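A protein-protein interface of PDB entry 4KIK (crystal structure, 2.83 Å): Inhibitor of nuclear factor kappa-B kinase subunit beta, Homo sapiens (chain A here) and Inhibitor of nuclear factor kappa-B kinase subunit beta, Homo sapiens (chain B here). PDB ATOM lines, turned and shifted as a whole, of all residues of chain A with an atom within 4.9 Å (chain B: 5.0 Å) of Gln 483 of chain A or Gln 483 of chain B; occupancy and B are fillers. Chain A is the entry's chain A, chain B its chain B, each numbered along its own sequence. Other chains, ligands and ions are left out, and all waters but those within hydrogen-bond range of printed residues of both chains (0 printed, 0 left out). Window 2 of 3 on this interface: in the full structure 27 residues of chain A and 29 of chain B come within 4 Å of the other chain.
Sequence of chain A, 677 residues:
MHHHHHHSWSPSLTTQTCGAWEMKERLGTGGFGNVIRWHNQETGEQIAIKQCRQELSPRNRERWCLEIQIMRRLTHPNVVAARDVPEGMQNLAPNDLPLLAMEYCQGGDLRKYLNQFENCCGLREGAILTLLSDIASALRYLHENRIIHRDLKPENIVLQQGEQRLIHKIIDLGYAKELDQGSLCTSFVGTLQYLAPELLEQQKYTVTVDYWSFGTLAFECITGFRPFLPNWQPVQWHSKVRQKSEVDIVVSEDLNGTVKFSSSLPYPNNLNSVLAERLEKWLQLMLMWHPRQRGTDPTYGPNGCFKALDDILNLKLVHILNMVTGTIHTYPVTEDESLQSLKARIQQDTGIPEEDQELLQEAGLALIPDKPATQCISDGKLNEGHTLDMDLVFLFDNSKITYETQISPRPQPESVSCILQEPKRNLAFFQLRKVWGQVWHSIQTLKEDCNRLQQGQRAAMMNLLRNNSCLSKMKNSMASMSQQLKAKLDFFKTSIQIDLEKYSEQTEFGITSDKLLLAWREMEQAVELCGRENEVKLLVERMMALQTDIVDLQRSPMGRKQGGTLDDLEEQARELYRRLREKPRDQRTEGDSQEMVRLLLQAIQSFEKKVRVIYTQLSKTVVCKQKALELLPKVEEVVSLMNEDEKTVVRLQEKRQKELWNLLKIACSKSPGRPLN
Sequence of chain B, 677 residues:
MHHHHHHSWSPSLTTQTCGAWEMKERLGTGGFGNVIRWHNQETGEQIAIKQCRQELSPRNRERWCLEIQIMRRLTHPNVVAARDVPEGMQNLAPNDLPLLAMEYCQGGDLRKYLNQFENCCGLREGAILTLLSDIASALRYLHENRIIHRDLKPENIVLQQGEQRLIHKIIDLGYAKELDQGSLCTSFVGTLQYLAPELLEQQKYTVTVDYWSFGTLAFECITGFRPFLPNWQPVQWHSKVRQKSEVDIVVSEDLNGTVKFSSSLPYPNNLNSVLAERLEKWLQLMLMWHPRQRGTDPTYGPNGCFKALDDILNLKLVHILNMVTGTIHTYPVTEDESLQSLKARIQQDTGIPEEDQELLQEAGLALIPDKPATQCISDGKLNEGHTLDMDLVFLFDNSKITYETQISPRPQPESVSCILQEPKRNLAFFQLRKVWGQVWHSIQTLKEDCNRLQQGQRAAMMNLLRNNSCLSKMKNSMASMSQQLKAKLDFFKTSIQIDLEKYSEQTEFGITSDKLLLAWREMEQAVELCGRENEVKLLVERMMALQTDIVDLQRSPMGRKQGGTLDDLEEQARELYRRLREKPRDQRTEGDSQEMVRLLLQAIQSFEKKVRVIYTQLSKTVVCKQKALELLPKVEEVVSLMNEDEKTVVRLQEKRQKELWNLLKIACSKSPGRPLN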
ATOM      1  N   ALA A 479      16.225   6.063   4.435  1.00  0.00           N
ATOM      2  CA  ALA A 479      15.207   7.093   4.169  1.00  0.00           C
ATOM      3  C   ALA A 479      15.642   8.454   4.722  1.00  0.00           C
ATOM      4  O   ALA A 479      15.647   9.437   3.989  1.00  0.00           O
ATOM      5  CB  ALA A 479      13.883   6.683   4.782  1.00  0.00           C
ATOM      6  N   SER A 480      16.060   8.482   5.995  1.00  0.00           N
ATOM      7  CA  SER A 480      16.546   9.654   6.725  1.00  0.00           C
ATOM      8  C   SER A 480      17.816  10.223   6.076  1.00  0.00           C
ATOM      9  O   SER A 480      17.898  11.435   5.903  1.00  0.00           O
ATOM     10  CB  SER A 480      16.810   9.287   8.183  1.00  0.00           C
ATOM     11  OG  SER A 480      17.349  10.348   8.951  1.00  0.00           O
ATOM     12  N   MET A 481      18.775   9.366   5.686  1.00  0.00           N
ATOM     13  CA  MET A 481      20.021   9.792   5.058  1.00  0.00           C
ATOM     14  C   MET A 481      19.782  10.375   3.683  1.00  0.00           C
ATOM     15  O   MET A 481      20.413  11.369   3.337  1.00  0.00           O
ATOM     16  CB  MET A 481      21.016   8.648   4.997  1.00  0.00           C
ATOM     17  CG  MET A 481      22.237   8.863   5.930  1.00  0.00           C
ATOM     18  SD  MET A 481      22.062   9.865   7.519  1.00  0.00           S
ATOM     19  CE  MET A 481      20.931   8.802   8.535  1.00  0.00           C
ATOM     20  N   SER A 482      18.814   9.811   2.944  1.00  0.00           N
ATOM     21  CA  SER A 482      18.404  10.257   1.619  1.00  0.00           C
ATOM     22  C   SER A 482      17.781  11.635   1.672  1.00  0.00           C
ATOM     23  O   SER A 482      18.000  12.428   0.757  1.00  0.00           O
ATOM     24  CB  SER A 482      17.425   9.266   0.990  1.00  0.00           C
ATOM     25  OG  SER A 482      17.350   9.475  -0.416  1.00  0.00           O
ATOM     26  N   GLN A 483      16.989  11.913   2.730  1.00  0.00           N
ATOM     27  CA  GLN A 483      16.313  13.197   2.936  1.00  0.00           C
ATOM     28  C   GLN A 483      17.322  14.255   3.325  1.00  0.00           C
ATOM     29  O   GLN A 483      17.250  15.372   2.810  1.00  0.00           O
ATOM     30  CB  GLN A 483      15.193  13.089   3.965  1.00  0.00           C
ATOM     31  CG  GLN A 483      13.871  12.739   3.307  1.00  0.00           C
ATOM     32  CD  GLN A 483      13.207  11.561   3.969  1.00  0.00           C
ATOM     33  OE1 GLN A 483      13.045  11.506   5.199  1.00  0.00           O
ATOM     34  NE2 GLN A 483      12.787  10.592   3.160  1.00  0.00           N
ATOM     35  N   GLN A 484      18.316  13.880   4.157  1.00  0.00           N
ATOM     36  CA  GLN A 484      19.410  14.750   4.570  1.00  0.00           C
ATOM     37  C   GLN A 484      20.291  15.058   3.381  1.00  0.00           C
ATOM     38  O   GLN A 484      20.720  16.198   3.240  1.00  0.00           O
ATOM     39  CB  GLN A 484      20.218  14.121   5.703  1.00  0.00           C
ATOM     40  CG  GLN A 484      19.547  14.266   7.056  1.00  0.00           C
ATOM     41  CD  GLN A 484      20.334  13.611   8.170  1.00  0.00           C
ATOM     42  OE1 GLN A 484      21.070  14.254   8.918  1.00  0.00           O
ATOM     43  NE2 GLN A 484      20.191  12.301   8.312  1.00  0.00           N
ATOM     44  N   LEU A 485      20.512  14.081   2.493  1.00  0.00           N
ATOM     45  CA  LEU A 485      21.330  14.303   1.307  1.00  0.00           C
ATOM     46  C   LEU A 485      20.605  15.201   0.329  1.00  0.00           C
ATOM     47  O   LEU A 485      21.230  16.123  -0.202  1.00  0.00           O
ATOM     48  CB  LEU A 485      21.749  12.984   0.625  1.00  0.00           C
ATOM     49  CG  LEU A 485      22.771  13.069  -0.522  1.00  0.00           C
ATOM     50  CD1 LEU A 485      24.130  13.582  -0.046  1.00  0.00           C
ATOM     51  CD2 LEU A 485      22.952  11.734  -1.165  1.00  0.00           C
ATOM     52  N   LYS A 486      19.296  14.974   0.116  1.00  0.00           N
ATOM     53  CA  LYS A 486      18.493  15.800  -0.796  1.00  0.00           C
ATOM     54  C   LYS A 486      18.597  17.280  -0.367  1.00  0.00           C
ATOM     55  O   LYS A 486      18.801  18.161  -1.214  1.00  0.00           O
ATOM     56  CB  LYS A 486      17.024  15.312  -0.826  1.00  0.00           C
ATOM     57  CG  LYS A 486      16.145  15.977  -1.897  1.00  0.00           C
ATOM     58  CD  LYS A 486      14.766  16.418  -1.330  1.00  0.00           C
ATOM     59  CE  LYS A 486      13.680  15.343  -1.412  1.00  0.00           C
ATOM     60  NZ  LYS A 486      13.119  14.935  -0.078  1.00  0.00           N
ATOM     61  N   ALA A 487      18.543  17.515   0.958  1.00  0.00           N
ATOM     62  CA  ALA A 487      18.616  18.821   1.595  1.00  0.00           C
ATOM     63  C   ALA A 487      19.990  19.491   1.394  1.00  0.00           C
ATOM     64  O   ALA A 487      20.039  20.667   1.015  1.00  0.00           O
ATOM     65  CB  ALA A 487      18.306  18.695   3.077  1.00  0.00           C
ATOM     66  N   ALA B 479       8.386  14.235   9.931  1.00  0.00           N
ATOM     67  CA  ALA B 479       9.627  13.464  10.060  1.00  0.00           C
ATOM     68  C   ALA B 479      10.628  13.826   8.942  1.00  0.00           C
ATOM     69  O   ALA B 479      11.776  14.163   9.228  1.00  0.00           O
ATOM     70  CB  ALA B 479       9.310  11.989  10.013  1.00  0.00           C
ATOM     71  N   SER B 480      10.156  13.823   7.687  1.00  0.00           N
ATOM     72  CA  SER B 480      10.915  14.161   6.490  1.00  0.00           C
ATOM     73  C   SER B 480      11.439  15.611   6.541  1.00  0.00           C
ATOM     74  O   SER B 480      12.613  15.844   6.247  1.00  0.00           O
ATOM     75  CB  SER B 480      10.034  13.943   5.258  1.00  0.00           C
ATOM     76  OG  SER B 480      10.678  14.241   4.029  1.00  0.00           O
ATOM     77  N   MET B 481      10.572  16.574   6.938  1.00  0.00           N
ATOM     78  CA  MET B 481      10.914  18.008   7.044  1.00  0.00           C
ATOM     79  C   MET B 481      11.978  18.243   8.107  1.00  0.00           C
ATOM     80  O   MET B 481      12.894  19.053   7.898  1.00  0.00           O
ATOM     81  CB  MET B 481       9.673  18.831   7.386  1.00  0.00           C
ATOM     82  CG  MET B 481       9.307  19.873   6.361  1.00  0.00           C
ATOM     83  SD  MET B 481       8.005  20.991   7.046  1.00  0.00           S
ATOM     84  CE  MET B 481       6.443  19.974   6.657  1.00  0.00           C
ATOM     85  N   SER B 482      11.879  17.487   9.221  1.00  0.00           N
ATOM     86  CA  SER B 482      12.797  17.530  10.341  1.00  0.00           C
ATOM     87  C   SER B 482      14.190  17.058   9.963  1.00  0.00           C
ATOM     88  O   SER B 482      15.179  17.614  10.445  1.00  0.00           O
ATOM     89  CB  SER B 482      12.270  16.676  11.479  1.00  0.00           C
ATOM     90  OG  SER B 482      12.995  16.974  12.656  1.00  0.00           O
ATOM     91  N   GLN B 483      14.272  16.018   9.130  1.00  0.00           N
ATOM     92  CA  GLN B 483      15.537  15.446   8.683  1.00  0.00           C
ATOM     93  C   GLN B 483      16.209  16.381   7.696  1.00  0.00           C
ATOM     94  O   GLN B 483      17.415  16.603   7.790  1.00  0.00           O
ATOM     95  CB  GLN B 483      15.318  14.058   8.089  1.00  0.00           C
ATOM     96  CG  GLN B 483      15.424  12.967   9.132  1.00  0.00           C
ATOM     97  CD  GLN B 483      14.250  12.027   9.076  1.00  0.00           C
ATOM     98  OE1 GLN B 483      13.865  11.508   8.012  1.00  0.00           O
ATOM     99  NE2 GLN B 483      13.682  11.753  10.242  1.00  0.00           N
ATOM    100  N   GLN B 484      15.405  17.013   6.826  1.00  0.00           N
ATOM    101  CA  GLN B 484      15.875  17.991   5.861  1.00  0.00           C
ATOM    102  C   GLN B 484      16.356  19.240   6.586  1.00  0.00           C
ATOM    103  O   GLN B 484      17.391  19.794   6.204  1.00  0.00           O
ATOM    104  CB  GLN B 484      14.774  18.303   4.842  1.00  0.00           C
ATOM    105  CG  GLN B 484      14.661  17.179   3.837  1.00  0.00           C
ATOM    106  CD  GLN B 484      13.674  17.383   2.750  1.00  0.00           C
ATOM    107  OE1 GLN B 484      12.584  16.804   2.765  1.00  0.00           O
ATOM    108  NE2 GLN B 484      14.125  18.034   1.686  1.00  0.00           N
ATOM    109  N   LEU B 485      15.652  19.649   7.673  1.00  0.00           N
ATOM    110  CA  LEU B 485      16.054  20.835   8.433  1.00  0.00           C
ATOM    111  C   LEU B 485      17.345  20.558   9.184  1.00  0.00           C
ATOM    112  O   LEU B 485      18.239  21.403   9.176  1.00  0.00           O
ATOM    113  CB  LEU B 485      14.950  21.328   9.380  1.00  0.00           C
ATOM    114  CG  LEU B 485      15.211  22.653  10.163  1.00  0.00           C
ATOM    115  CD1 LEU B 485      15.270  23.872   9.248  1.00  0.00           C
ATOM    116  CD2 LEU B 485      14.177  22.866  11.242  1.00  0.00           C
ATOM    117  N   LYS B 486      17.461  19.380   9.802  1.00  0.00           N
ATOM    118  CA  LYS B 486      18.663  19.003  10.551  1.00  0.00           C
ATOM    119  C   LYS B 486      19.881  19.145   9.636  1.00  0.00           C
ATOM    120  O   LYS B 486      20.894  19.711  10.050  1.00  0.00           O
ATOM    121  CB  LYS B 486      18.534  17.560  11.114  1.00  0.00           C
ATOM    122  CG  LYS B 486      19.605  17.182  12.132  1.00  0.00           C
ATOM    123  CD  LYS B 486      20.180  15.783  11.882  1.00  0.00           C
ATOM    124  CE  LYS B 486      19.408  14.693  12.599  1.00  0.00           C
ATOM    125  NZ  LYS B 486      20.130  13.397  12.571  1.00  0.00           N
ATOM    126  N   ALA B 487      19.727  18.703   8.370  1.00  0.00           N
ATOM    127  CA  ALA B 487      20.748  18.718   7.333  1.00  0.00           C
ATOM    128  C   ALA B 487      21.143  20.146   6.933  1.00  0.00           C
ATOM    129  O   ALA B 487      22.342  20.446   6.891  1.00  0.00           O
ATOM    130  CB  ALA B 487      20.255  17.952   6.115  1.00  0.00           C
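OE1 of Gln 483 of chain B lies close to OE1 of Gln 483 of chain A (2.9 Å). OE1 of Gln 484 of chain B lies within hydrogen-bond range of NZ of Lys 486 of chain A (3.4 Å).
Of the printed residues of chain B, Gln 483 of chain A touches Ser 480 (3.6 Å), Gln 483 (2.9 Å) and Gln 484 (3.3 Å). Gln 483 of chain B touches three residues of chain A. Printed residues of chain A within 4 Å of Gln 484 of chain B: Gln 483, Lys 486 and Ala 487. Printed residues of chain A within 4 Å of Ser 480 of chain B: Gln 483. The nearest residue of chain A that does not touch Gln 483 of chain B is Ala 479 of chain A (4.8 Å).
Printed residues of chain B that touch a printed residue of chain A: Ser 480, Gln 483, Gln 484, Lys 486 and Ala 487. Hydrophobic or aromatic side chains of chain B that line the printed part of chain A: Ala 487. Among the printed residues, no Asp or Glu carboxylate lies within 4 Å of a Lys or Arg side-chain nitrogen of the other chain.
Gln 483 of chain B touches Ser 480 of chain A (CG to OG, 3.3 Å). CG of Gln 483 of chain A touches OG of Ser 480 of chain B, 3.6 Å away. CG of Gln 484 of chain B touches O of Gln 483 of chain A (3.3 Å). Gln 484 of chain A touches Gln 483 of chain B (CG to O, 3.2 Å). Gln 484 of chain A touches Lys 486 of chain B (OE1 to CD, 3.5 Å). Gln 484 of chain A touches Ala 487 of chain B (O to CB, 3.4 Å). Gln 484 of chain B touches Ala 487 of chain A (O to CB, 3.4 Å). CB of Ala 487 of chain A touches CB of Ala 487 of chain B, 3.7 Å away.
The side-chain amide nitrogen of Gln 484 of chain A lies within hydrogen-bond range of the backbone carbonyl oxygen of Ser 480 of chain A (3.4 Å). The side-chain amide oxygen of Gln 484 of chain B is in hydrogen-bond range of the side-chain hydroxyl of Ser 480 of chain B (3.4 Å). O of Ala 479 of chain B is in hydrogen-bond range of NE2 of Gln 483 of chain B, at 3.2 Å. NE2 of Gln 483 of chain A sits at hydrogen-bond distance from O of Ala 479 of chain A (3.2 Å). The side-chain sulfur (SD) of Met 481 of chain A lies within hydrogen-bond range of the side-chain amide nitrogen (NE2) of Gln 484 of chain A, 3.2 Å away.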
